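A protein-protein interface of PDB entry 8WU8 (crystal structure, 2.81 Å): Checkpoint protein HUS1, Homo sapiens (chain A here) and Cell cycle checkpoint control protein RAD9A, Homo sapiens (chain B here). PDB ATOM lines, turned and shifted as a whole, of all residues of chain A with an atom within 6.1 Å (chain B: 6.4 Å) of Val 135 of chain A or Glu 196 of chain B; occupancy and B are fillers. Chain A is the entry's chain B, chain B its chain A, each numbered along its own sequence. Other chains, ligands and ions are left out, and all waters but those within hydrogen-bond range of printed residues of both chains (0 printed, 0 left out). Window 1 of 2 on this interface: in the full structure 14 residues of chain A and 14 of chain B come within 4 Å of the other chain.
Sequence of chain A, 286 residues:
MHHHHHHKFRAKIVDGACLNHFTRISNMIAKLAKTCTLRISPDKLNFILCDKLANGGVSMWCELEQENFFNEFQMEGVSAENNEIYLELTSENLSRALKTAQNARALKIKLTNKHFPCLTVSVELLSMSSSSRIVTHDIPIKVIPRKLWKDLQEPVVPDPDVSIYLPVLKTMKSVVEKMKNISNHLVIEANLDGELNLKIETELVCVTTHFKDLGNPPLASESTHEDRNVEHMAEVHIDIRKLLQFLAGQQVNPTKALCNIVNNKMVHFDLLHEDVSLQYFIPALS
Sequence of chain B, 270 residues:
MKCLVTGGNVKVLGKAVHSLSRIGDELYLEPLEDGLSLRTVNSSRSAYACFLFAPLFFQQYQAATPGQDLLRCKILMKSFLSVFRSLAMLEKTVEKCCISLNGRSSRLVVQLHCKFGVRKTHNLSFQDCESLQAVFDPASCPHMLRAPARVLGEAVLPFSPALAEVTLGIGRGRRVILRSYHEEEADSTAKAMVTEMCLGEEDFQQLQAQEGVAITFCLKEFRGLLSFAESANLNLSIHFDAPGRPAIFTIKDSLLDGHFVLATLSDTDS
OG1 of Thr 195 of chain B is in hydrogen-bond range of ND1 of His 137 of chain A. The backbone carbonyl oxygen of Ile 134 of chain A lies within hydrogen-bond range of the backbone NH of Cys 198 of chain B, at 3.0 Å. The backbone carbonyl oxygen (O) of Glu 196 of chain B is in hydrogen-bond range of the backbone NH (N) of Thr 136 of chain A (2.9 Å). The backbone carbonyl oxygen of Thr 136 of chain A sits close to the backbone carbonyl oxygen of Val 194 of chain B.
The backbone carbonyl oxygen of Met 197 of chain B sits at hydrogen-bond distance from the backbone NH of Leu 178 of chain B (2.7 Å). The backbone NH (N) of Val 121 of chain A is in hydrogen-bond range of the backbone carbonyl oxygen (O) of His 137 of chain A, at 3.0 Å. OE1 of Glu 196 of chain B is in salt-bridge range of NE of Arg 179 of chain B, at 3.6 Å. The backbone NH (N) of Val 123 of chain A sits at hydrogen-bond distance from the backbone carbonyl oxygen (O) of Val 135 of chain A (2.9 Å). The backbone NH of Ser 180 of chain B is in hydrogen-bond range of the backbone carbonyl oxygen of Thr 195 of chain B. The backbone NH of Leu 125 of chain A is in hydrogen-bond range of the backbone carbonyl oxygen of Arg 133 of chain A, at 2.7 Å.
Among the printed residues, pairs that only touch across the chains: Thr 136 of chain A with Thr 195 of chain B (3.3 Å), Val 135 of chain A with Glu 196 of chain B (3.3 Å), His 137 of chain A with Val 194 of chain B (3.4 Å), Thr 100 of chain A with Pro 158 of chain B (3.5 Å), Val 135 of chain A with Met 197 of chain B (3.5 Å), His 137 of chain A with Pro 158 of chain B (3.6 Å), Ile 134 of chain A with Glu 196 of chain B (3.6 Å), Val 135 of chain A with Pro 158 of chain B (3.6 Å), Ile 134 of chain A with Met 197 of chain B (3.7 Å), Val 135 of chain A with Thr 195 of chain B (3.8 Å), Arg 133 of chain A with Cys 198 of chain B (3.8 Å) and Arg 133 of chain A with Met 197 of chain B (3.8 Å).
Of the printed residues of chain B, Thr 100 of chain A touches Pro 158. Printed residues of chain A within 4 Å of Val 194 of chain B: Thr 136 (3.4 Å) and His 137 (3.4 Å). Glu 196 of chain B touches three residues of chain A. Printed residues of chain A within 4 Å of Met 197 of chain B: Arg 133 (3.8 Å), Ile 134 (3.7 Å) and Val 135 (3.5 Å). The nearest residue of chain B that does not touch Val 135 of chain A is Cys 198 of chain B (5.0 Å).
Of the 11 printed residues of chain B, 6 touch a printed residue of chain A. Hydrophobic or aromatic side chains of chain B that line the printed part of chain A: Pro 158 and Met 197. Of the 11 printed residues of chain A, 6 touch a printed residue of chain B. Printed residues of chain A that touch a printed residue of chain B: Thr 100, Arg 133, Ile 134, Val 135, Thr 136 and His 137. Hydrophobic or aromatic side chains of chain A that line the printed part of chain B: Val 135 and His 137. Among the printed residues, 16 pairs touch across the chains. Among the printed residues, no Asp or Glu carboxylate lies within 4 Å of a Lys or Arg side-chain nitrogen of the other chain.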
ATOM      1  N   THR A 100     -10.046 -17.913  17.142  1.00  0.00           N
ATOM      2  CA  THR A 100     -11.419 -17.588  16.775  1.00  0.00           C
ATOM      3  C   THR A 100     -11.866 -18.409  15.564  1.00  0.00           C
ATOM      4  O   THR A 100     -13.041 -18.760  15.429  1.00  0.00           O
ATOM      5  CB  THR A 100     -11.570 -16.081  16.462  1.00  0.00           C
ATOM      6  OG1 THR A 100     -11.106 -15.314  17.578  1.00  0.00           O
ATOM      7  CG2 THR A 100     -13.020 -15.725  16.173  1.00  0.00           C
ATOM      8  N   VAL A 121      -6.281  -9.701  10.551  1.00  0.00           N
ATOM      9  CA  VAL A 121      -6.852 -11.015  10.308  1.00  0.00           C
ATOM     10  C   VAL A 121      -8.369 -10.919  10.288  1.00  0.00           C
ATOM     11  O   VAL A 121      -8.991 -10.644  11.315  1.00  0.00           O
ATOM     12  CB  VAL A 121      -6.412 -12.026  11.379  1.00  0.00           C
ATOM     13  CG1 VAL A 121      -7.000 -13.402  11.093  1.00  0.00           C
ATOM     14  CG2 VAL A 121      -4.896 -12.076  11.457  1.00  0.00           C
ATOM     15  N   SER A 122      -8.955 -11.130   9.113  1.00  0.00           N
ATOM     16  CA  SER A 122     -10.406 -11.148   8.967  1.00  0.00           C
ATOM     17  C   SER A 122     -10.922 -12.576   9.036  1.00  0.00           C
ATOM     18  O   SER A 122     -10.356 -13.477   8.418  1.00  0.00           O
ATOM     19  CB  SER A 122     -10.829 -10.501   7.648  1.00  0.00           C
ATOM     20  OG  SER A 122     -10.449  -9.139   7.609  1.00  0.00           O
ATOM     21  N   VAL A 123     -11.994 -12.784   9.790  1.00  0.00           N
ATOM     22  CA  VAL A 123     -12.554 -14.121   9.944  1.00  0.00           C
ATOM     23  C   VAL A 123     -14.049 -14.149   9.647  1.00  0.00           C
ATOM     24  O   VAL A 123     -14.830 -13.436  10.276  1.00  0.00           O
ATOM     25  CB  VAL A 123     -12.327 -14.673  11.367  1.00  0.00           C
ATOM     26  CG1 VAL A 123     -12.947 -16.058  11.508  1.00  0.00           C
ATOM     27  CG2 VAL A 123     -10.841 -14.714  11.701  1.00  0.00           C
ATOM     28  N   GLU A 124     -14.439 -14.971   8.676  1.00  0.00           N
ATOM     29  CA  GLU A 124     -15.846 -15.282   8.456  1.00  0.00           C
ATOM     30  C   GLU A 124     -16.268 -16.366   9.428  1.00  0.00           C
ATOM     31  O   GLU A 124     -16.145 -17.553   9.127  1.00  0.00           O
ATOM     32  CB  GLU A 124     -16.106 -15.747   7.021  1.00  0.00           C
ATOM     33  CG  GLU A 124     -16.363 -14.631   6.024  1.00  0.00           C
ATOM     34  CD  GLU A 124     -17.172 -15.103   4.827  1.00  0.00           C
ATOM     35  OE1 GLU A 124     -17.582 -16.283   4.817  1.00  0.00           O
ATOM     36  OE2 GLU A 124     -17.402 -14.294   3.902  1.00  0.00           O
ATOM     37  N   LEU A 125     -16.859 -16.003  10.539  1.00  0.00           N
ATOM     38  CA  LEU A 125     -17.309 -17.038  11.429  1.00  0.00           C
ATOM     39  C   LEU A 125     -18.485 -17.812  10.877  1.00  0.00           C
ATOM     40  O   LEU A 125     -19.154 -17.373   9.963  1.00  0.00           O
ATOM     41  CB  LEU A 125     -17.624 -16.463  12.792  1.00  0.00           C
ATOM     42  CG  LEU A 125     -16.378 -16.181  13.603  1.00  0.00           C
ATOM     43  CD1 LEU A 125     -16.764 -15.928  15.041  1.00  0.00           C
ATOM     44  CD2 LEU A 125     -15.388 -17.322  13.518  1.00  0.00           C
ATOM     45  N   ARG A 133     -21.055 -13.737  10.335  1.00  0.00           N
ATOM     46  CA  ARG A 133     -20.411 -13.165  11.508  1.00  0.00           C
ATOM     47  C   ARG A 133     -18.971 -12.830  11.149  1.00  0.00           C
ATOM     48  O   ARG A 133     -18.181 -13.726  10.853  1.00  0.00           O
ATOM     49  CB  ARG A 133     -20.454 -14.134  12.690  1.00  0.00           C
ATOM     50  CG  ARG A 133     -21.770 -14.871  12.861  1.00  0.00           C
ATOM     51  CD  ARG A 133     -22.759 -14.064  13.677  1.00  0.00           C
ATOM     52  NE  ARG A 133     -23.893 -14.877  14.099  1.00  0.00           N
ATOM     53  CZ  ARG A 133     -23.859 -15.729  15.119  1.00  0.00           C
ATOM     54  NH1 ARG A 133     -22.746 -15.882  15.823  1.00  0.00           N
ATOM     55  NH2 ARG A 133     -24.939 -16.431  15.434  1.00  0.00           N
ATOM     56  N   ILE A 134     -18.627 -11.549  11.168  1.00  0.00           N
ATOM     57  CA  ILE A 134     -17.295 -11.130  10.745  1.00  0.00           C
ATOM     58  C   ILE A 134     -16.468 -10.531  11.875  1.00  0.00           C
ATOM     59  O   ILE A 134     -16.813  -9.486  12.423  1.00  0.00           O
ATOM     60  CB  ILE A 134     -17.375 -10.104   9.613  1.00  0.00           C
ATOM     61  CG1 ILE A 134     -18.301 -10.615   8.515  1.00  0.00           C
ATOM     62  CG2 ILE A 134     -15.988  -9.809   9.071  1.00  0.00           C
ATOM     63  CD1 ILE A 134     -17.874 -11.939   7.933  1.00  0.00           C
ATOM     64  N   VAL A 135     -15.367 -11.195  12.210  1.00  0.00           N
ATOM     65  CA  VAL A 135     -14.440 -10.675  13.206  1.00  0.00           C
ATOM     66  C   VAL A 135     -13.222 -10.068  12.528  1.00  0.00           C
ATOM     67  O   VAL A 135     -12.752 -10.571  11.508  1.00  0.00           O
ATOM     68  CB  VAL A 135     -13.976 -11.766  14.182  1.00  0.00           C
ATOM     69  CG1 VAL A 135     -13.387 -11.130  15.430  1.00  0.00           C
ATOM     70  CG2 VAL A 135     -15.133 -12.672  14.545  1.00  0.00           C
ATOM     71  N   THR A 136     -12.712  -8.983  13.098  1.00  0.00           N
ATOM     72  CA  THR A 136     -11.526  -8.342  12.557  1.00  0.00           C
ATOM     73  C   THR A 136     -10.542  -7.986  13.663  1.00  0.00           C
ATOM     74  O   THR A 136     -10.844  -7.182  14.550  1.00  0.00           O
ATOM     75  CB  THR A 136     -11.889  -7.081  11.768  1.00  0.00           C
ATOM     76  OG1 THR A 136     -12.829  -7.422  10.745  1.00  0.00           O
ATOM     77  CG2 THR A 136     -10.648  -6.478  11.132  1.00  0.00           C
ATOM     78  N   HIS A 137      -9.364  -8.598  13.605  1.00  0.00           N
ATOM     79  CA  HIS A 137      -8.308  -8.324  14.565  1.00  0.00           C
ATOM     80  C   HIS A 137      -7.215  -7.481  13.927  1.00  0.00           C
ATOM     81  O   HIS A 137      -6.573  -7.909  12.968  1.00  0.00           O
ATOM     82  CB  HIS A 137      -7.707  -9.624  15.098  1.00  0.00           C
ATOM     83  CG  HIS A 137      -8.715 -10.578  15.656  1.00  0.00           C
ATOM     84  ND1 HIS A 137      -8.971 -10.687  17.006  1.00  0.00           N
ATOM     85  CD2 HIS A 137      -9.529 -11.471  15.047  1.00  0.00           C
ATOM     86  CE1 HIS A 137      -9.900 -11.604  17.205  1.00  0.00           C
ATOM     87  NE2 HIS A 137     -10.256 -12.097  16.032  1.00  0.00           N
ATOM     88  N   PRO B 158     -14.651 -13.890  20.372  1.00  0.00           N
ATOM     89  CA  PRO B 158     -13.295 -13.536  19.928  1.00  0.00           C
ATOM     90  C   PRO B 158     -12.596 -12.461  20.766  1.00  0.00           C
ATOM     91  O   PRO B 158     -11.529 -11.992  20.362  1.00  0.00           O
ATOM     92  CB  PRO B 158     -13.522 -13.018  18.506  1.00  0.00           C
ATOM     93  CG  PRO B 158     -14.898 -12.478  18.528  1.00  0.00           C
ATOM     94  CD  PRO B 158     -15.671 -13.401  19.422  1.00  0.00           C
ATOM     95  N   PHE B 159     -13.179 -12.070  21.894  1.00  0.00           N
ATOM     96  CA  PHE B 159     -12.529 -11.106  22.774  1.00  0.00           C
ATOM     97  C   PHE B 159     -11.731 -11.806  23.856  1.00  0.00           C
ATOM     98  O   PHE B 159     -12.181 -12.801  24.423  1.00  0.00           O
ATOM     99  CB  PHE B 159     -13.549 -10.173  23.421  1.00  0.00           C
ATOM    100  CG  PHE B 159     -14.243  -9.268  22.453  1.00  0.00           C
ATOM    101  CD1 PHE B 159     -13.589  -8.169  21.924  1.00  0.00           C
ATOM    102  CD2 PHE B 159     -15.554  -9.512  22.076  1.00  0.00           C
ATOM    103  CE1 PHE B 159     -14.226  -7.332  21.030  1.00  0.00           C
ATOM    104  CE2 PHE B 159     -16.196  -8.681  21.188  1.00  0.00           C
ATOM    105  CZ  PHE B 159     -15.531  -7.587  20.662  1.00  0.00           C
ATOM    106  N   ILE B 177     -22.319  -3.912  15.923  1.00  0.00           N
ATOM    107  CA  ILE B 177     -20.863  -3.956  15.968  1.00  0.00           C
ATOM    108  C   ILE B 177     -20.319  -3.925  17.395  1.00  0.00           C
ATOM    109  O   ILE B 177     -20.670  -3.049  18.184  1.00  0.00           O
ATOM    110  CB  ILE B 177     -20.259  -2.785  15.176  1.00  0.00           C
ATOM    111  CG1 ILE B 177     -20.765  -2.807  13.734  1.00  0.00           C
ATOM    112  CG2 ILE B 177     -18.747  -2.843  15.211  1.00  0.00           C
ATOM    113  CD1 ILE B 177     -20.232  -1.684  12.884  1.00  0.00           C
ATOM    114  N   LEU B 178     -19.462  -4.890  17.719  1.00  0.00           N
ATOM    115  CA  LEU B 178     -18.766  -4.905  19.004  1.00  0.00           C
ATOM    116  C   LEU B 178     -17.276  -4.630  18.831  1.00  0.00           C
ATOM    117  O   LEU B 178     -16.535  -5.471  18.323  1.00  0.00           O
ATOM    118  CB  LEU B 178     -18.962  -6.244  19.715  1.00  0.00           C
ATOM    119  CG  LEU B 178     -20.343  -6.543  20.296  1.00  0.00           C
ATOM    120  CD1 LEU B 178     -20.317  -7.864  21.036  1.00  0.00           C
ATOM    121  CD2 LEU B 178     -20.783  -5.426  21.220  1.00  0.00           C
ATOM    122  N   ARG B 179     -16.843  -3.448  19.259  1.00  0.00           N
ATOM    123  CA  ARG B 179     -15.440  -3.057  19.179  1.00  0.00           C
ATOM    124  C   ARG B 179     -14.799  -3.124  20.556  1.00  0.00           C
ATOM    125  O   ARG B 179     -15.408  -2.720  21.545  1.00  0.00           O
ATOM    126  CB  ARG B 179     -15.308  -1.643  18.613  1.00  0.00           C
ATOM    127  CG  ARG B 179     -14.368  -1.500  17.431  1.00  0.00           C
ATOM    128  CD  ARG B 179     -14.421  -0.083  16.866  1.00  0.00           C
ATOM    129  NE  ARG B 179     -15.789   0.341  16.557  1.00  0.00           N
ATOM    130  CZ  ARG B 179     -16.472   1.250  17.249  1.00  0.00           C
ATOM    131  NH1 ARG B 179     -17.710   1.568  16.890  1.00  0.00           N
ATOM    132  NH2 ARG B 179     -15.918   1.849  18.297  1.00  0.00           N
ATOM    133  N   SER B 180     -13.576  -3.635  20.628  1.00  0.00           N
ATOM    134  CA  SER B 180     -12.852  -3.628  21.890  1.00  0.00           C
ATOM    135  C   SER B 180     -12.439  -2.195  22.203  1.00  0.00           C
ATOM    136  O   SER B 180     -12.185  -1.401  21.295  1.00  0.00           O
ATOM    137  CB  SER B 180     -11.639  -4.556  21.836  1.00  0.00           C
ATOM    138  OG  SER B 180     -10.746  -4.184  20.804  1.00  0.00           O
ATOM    139  N   VAL B 194      -6.669  -4.662  18.515  1.00  0.00           N
ATOM    140  CA  VAL B 194      -8.053  -4.212  18.428  1.00  0.00           C
ATOM    141  C   VAL B 194      -8.915  -5.254  17.719  1.00  0.00           C
ATOM    142  O   VAL B 194      -8.625  -5.647  16.586  1.00  0.00           O
ATOM    143  CB  VAL B 194      -8.163  -2.863  17.692  1.00  0.00           C
ATOM    144  CG1 VAL B 194      -9.617  -2.470  17.505  1.00  0.00           C
ATOM    145  CG2 VAL B 194      -7.407  -1.781  18.456  1.00  0.00           C
ATOM    146  N   THR B 195      -9.973  -5.698  18.393  1.00  0.00           N
ATOM    147  CA  THR B 195     -10.882  -6.699  17.843  1.00  0.00           C
ATOM    148  C   THR B 195     -12.283  -6.136  17.633  1.00  0.00           C
ATOM    149  O   THR B 195     -12.880  -5.575  18.555  1.00  0.00           O
ATOM    150  CB  THR B 195     -10.990  -7.920  18.760  1.00  0.00           C
ATOM    151  OG1 THR B 195      -9.689  -8.481  18.969  1.00  0.00           O
ATOM    152  CG2 THR B 195     -11.902  -8.963  18.147  1.00  0.00           C
ATOM    153  N   GLU B 196     -12.812  -6.297  16.425  1.00  0.00           N
ATOM    154  CA  GLU B 196     -14.164  -5.844  16.126  1.00  0.00           C
ATOM    155  C   GLU B 196     -15.052  -6.981  15.623  1.00  0.00           C
ATOM    156  O   GLU B 196     -14.701  -7.678  14.670  1.00  0.00           O
ATOM    157  CB  GLU B 196     -14.127  -4.714  15.098  1.00  0.00           C
ATOM    158  CG  GLU B 196     -15.494  -4.252  14.635  1.00  0.00           C
ATOM    159  CD  GLU B 196     -15.431  -3.028  13.744  1.00  0.00           C
ATOM    160  OE1 GLU B 196     -14.680  -2.088  14.082  1.00  0.00           O
ATOM    161  OE2 GLU B 196     -16.124  -3.011  12.703  1.00  0.00           O
ATOM    162  N   MET B 197     -16.201  -7.155  16.274  1.00  0.00           N
ATOM    163  CA  MET B 197     -17.189  -8.163  15.883  1.00  0.00           C
ATOM    164  C   MET B 197     -18.401  -7.528  15.212  1.00  0.00           C
ATOM    165  O   MET B 197     -18.924  -6.527  15.696  1.00  0.00           O
ATOM    166  CB  MET B 197     -17.634  -8.973  17.105  1.00  0.00           C
ATOM    167  CG  MET B 197     -18.727  -9.987  16.824  1.00  0.00           C
ATOM    168  SD  MET B 197     -18.176 -11.310  15.722  1.00  0.00           S
ATOM    169  CE  MET B 197     -19.465 -12.525  15.967  1.00  0.00           C
ATOM    170  N   CYS B 198     -18.856  -8.118  14.108  1.00  0.00           N
ATOM    171  CA  CYS B 198     -19.974  -7.554  13.351  1.00  0.00           C
ATOM    172  C   CYS B 198     -21.116  -8.550  13.130  1.00  0.00           C
ATOM    173  O   CYS B 198     -20.963  -9.534  12.405  1.00  0.00           O
ATOM    174  CB  CYS B 198     -19.486  -7.031  11.999  1.00  0.00           C
ATOM    175  SG  CYS B 198     -20.788  -6.333  10.959  1.00  0.00           S
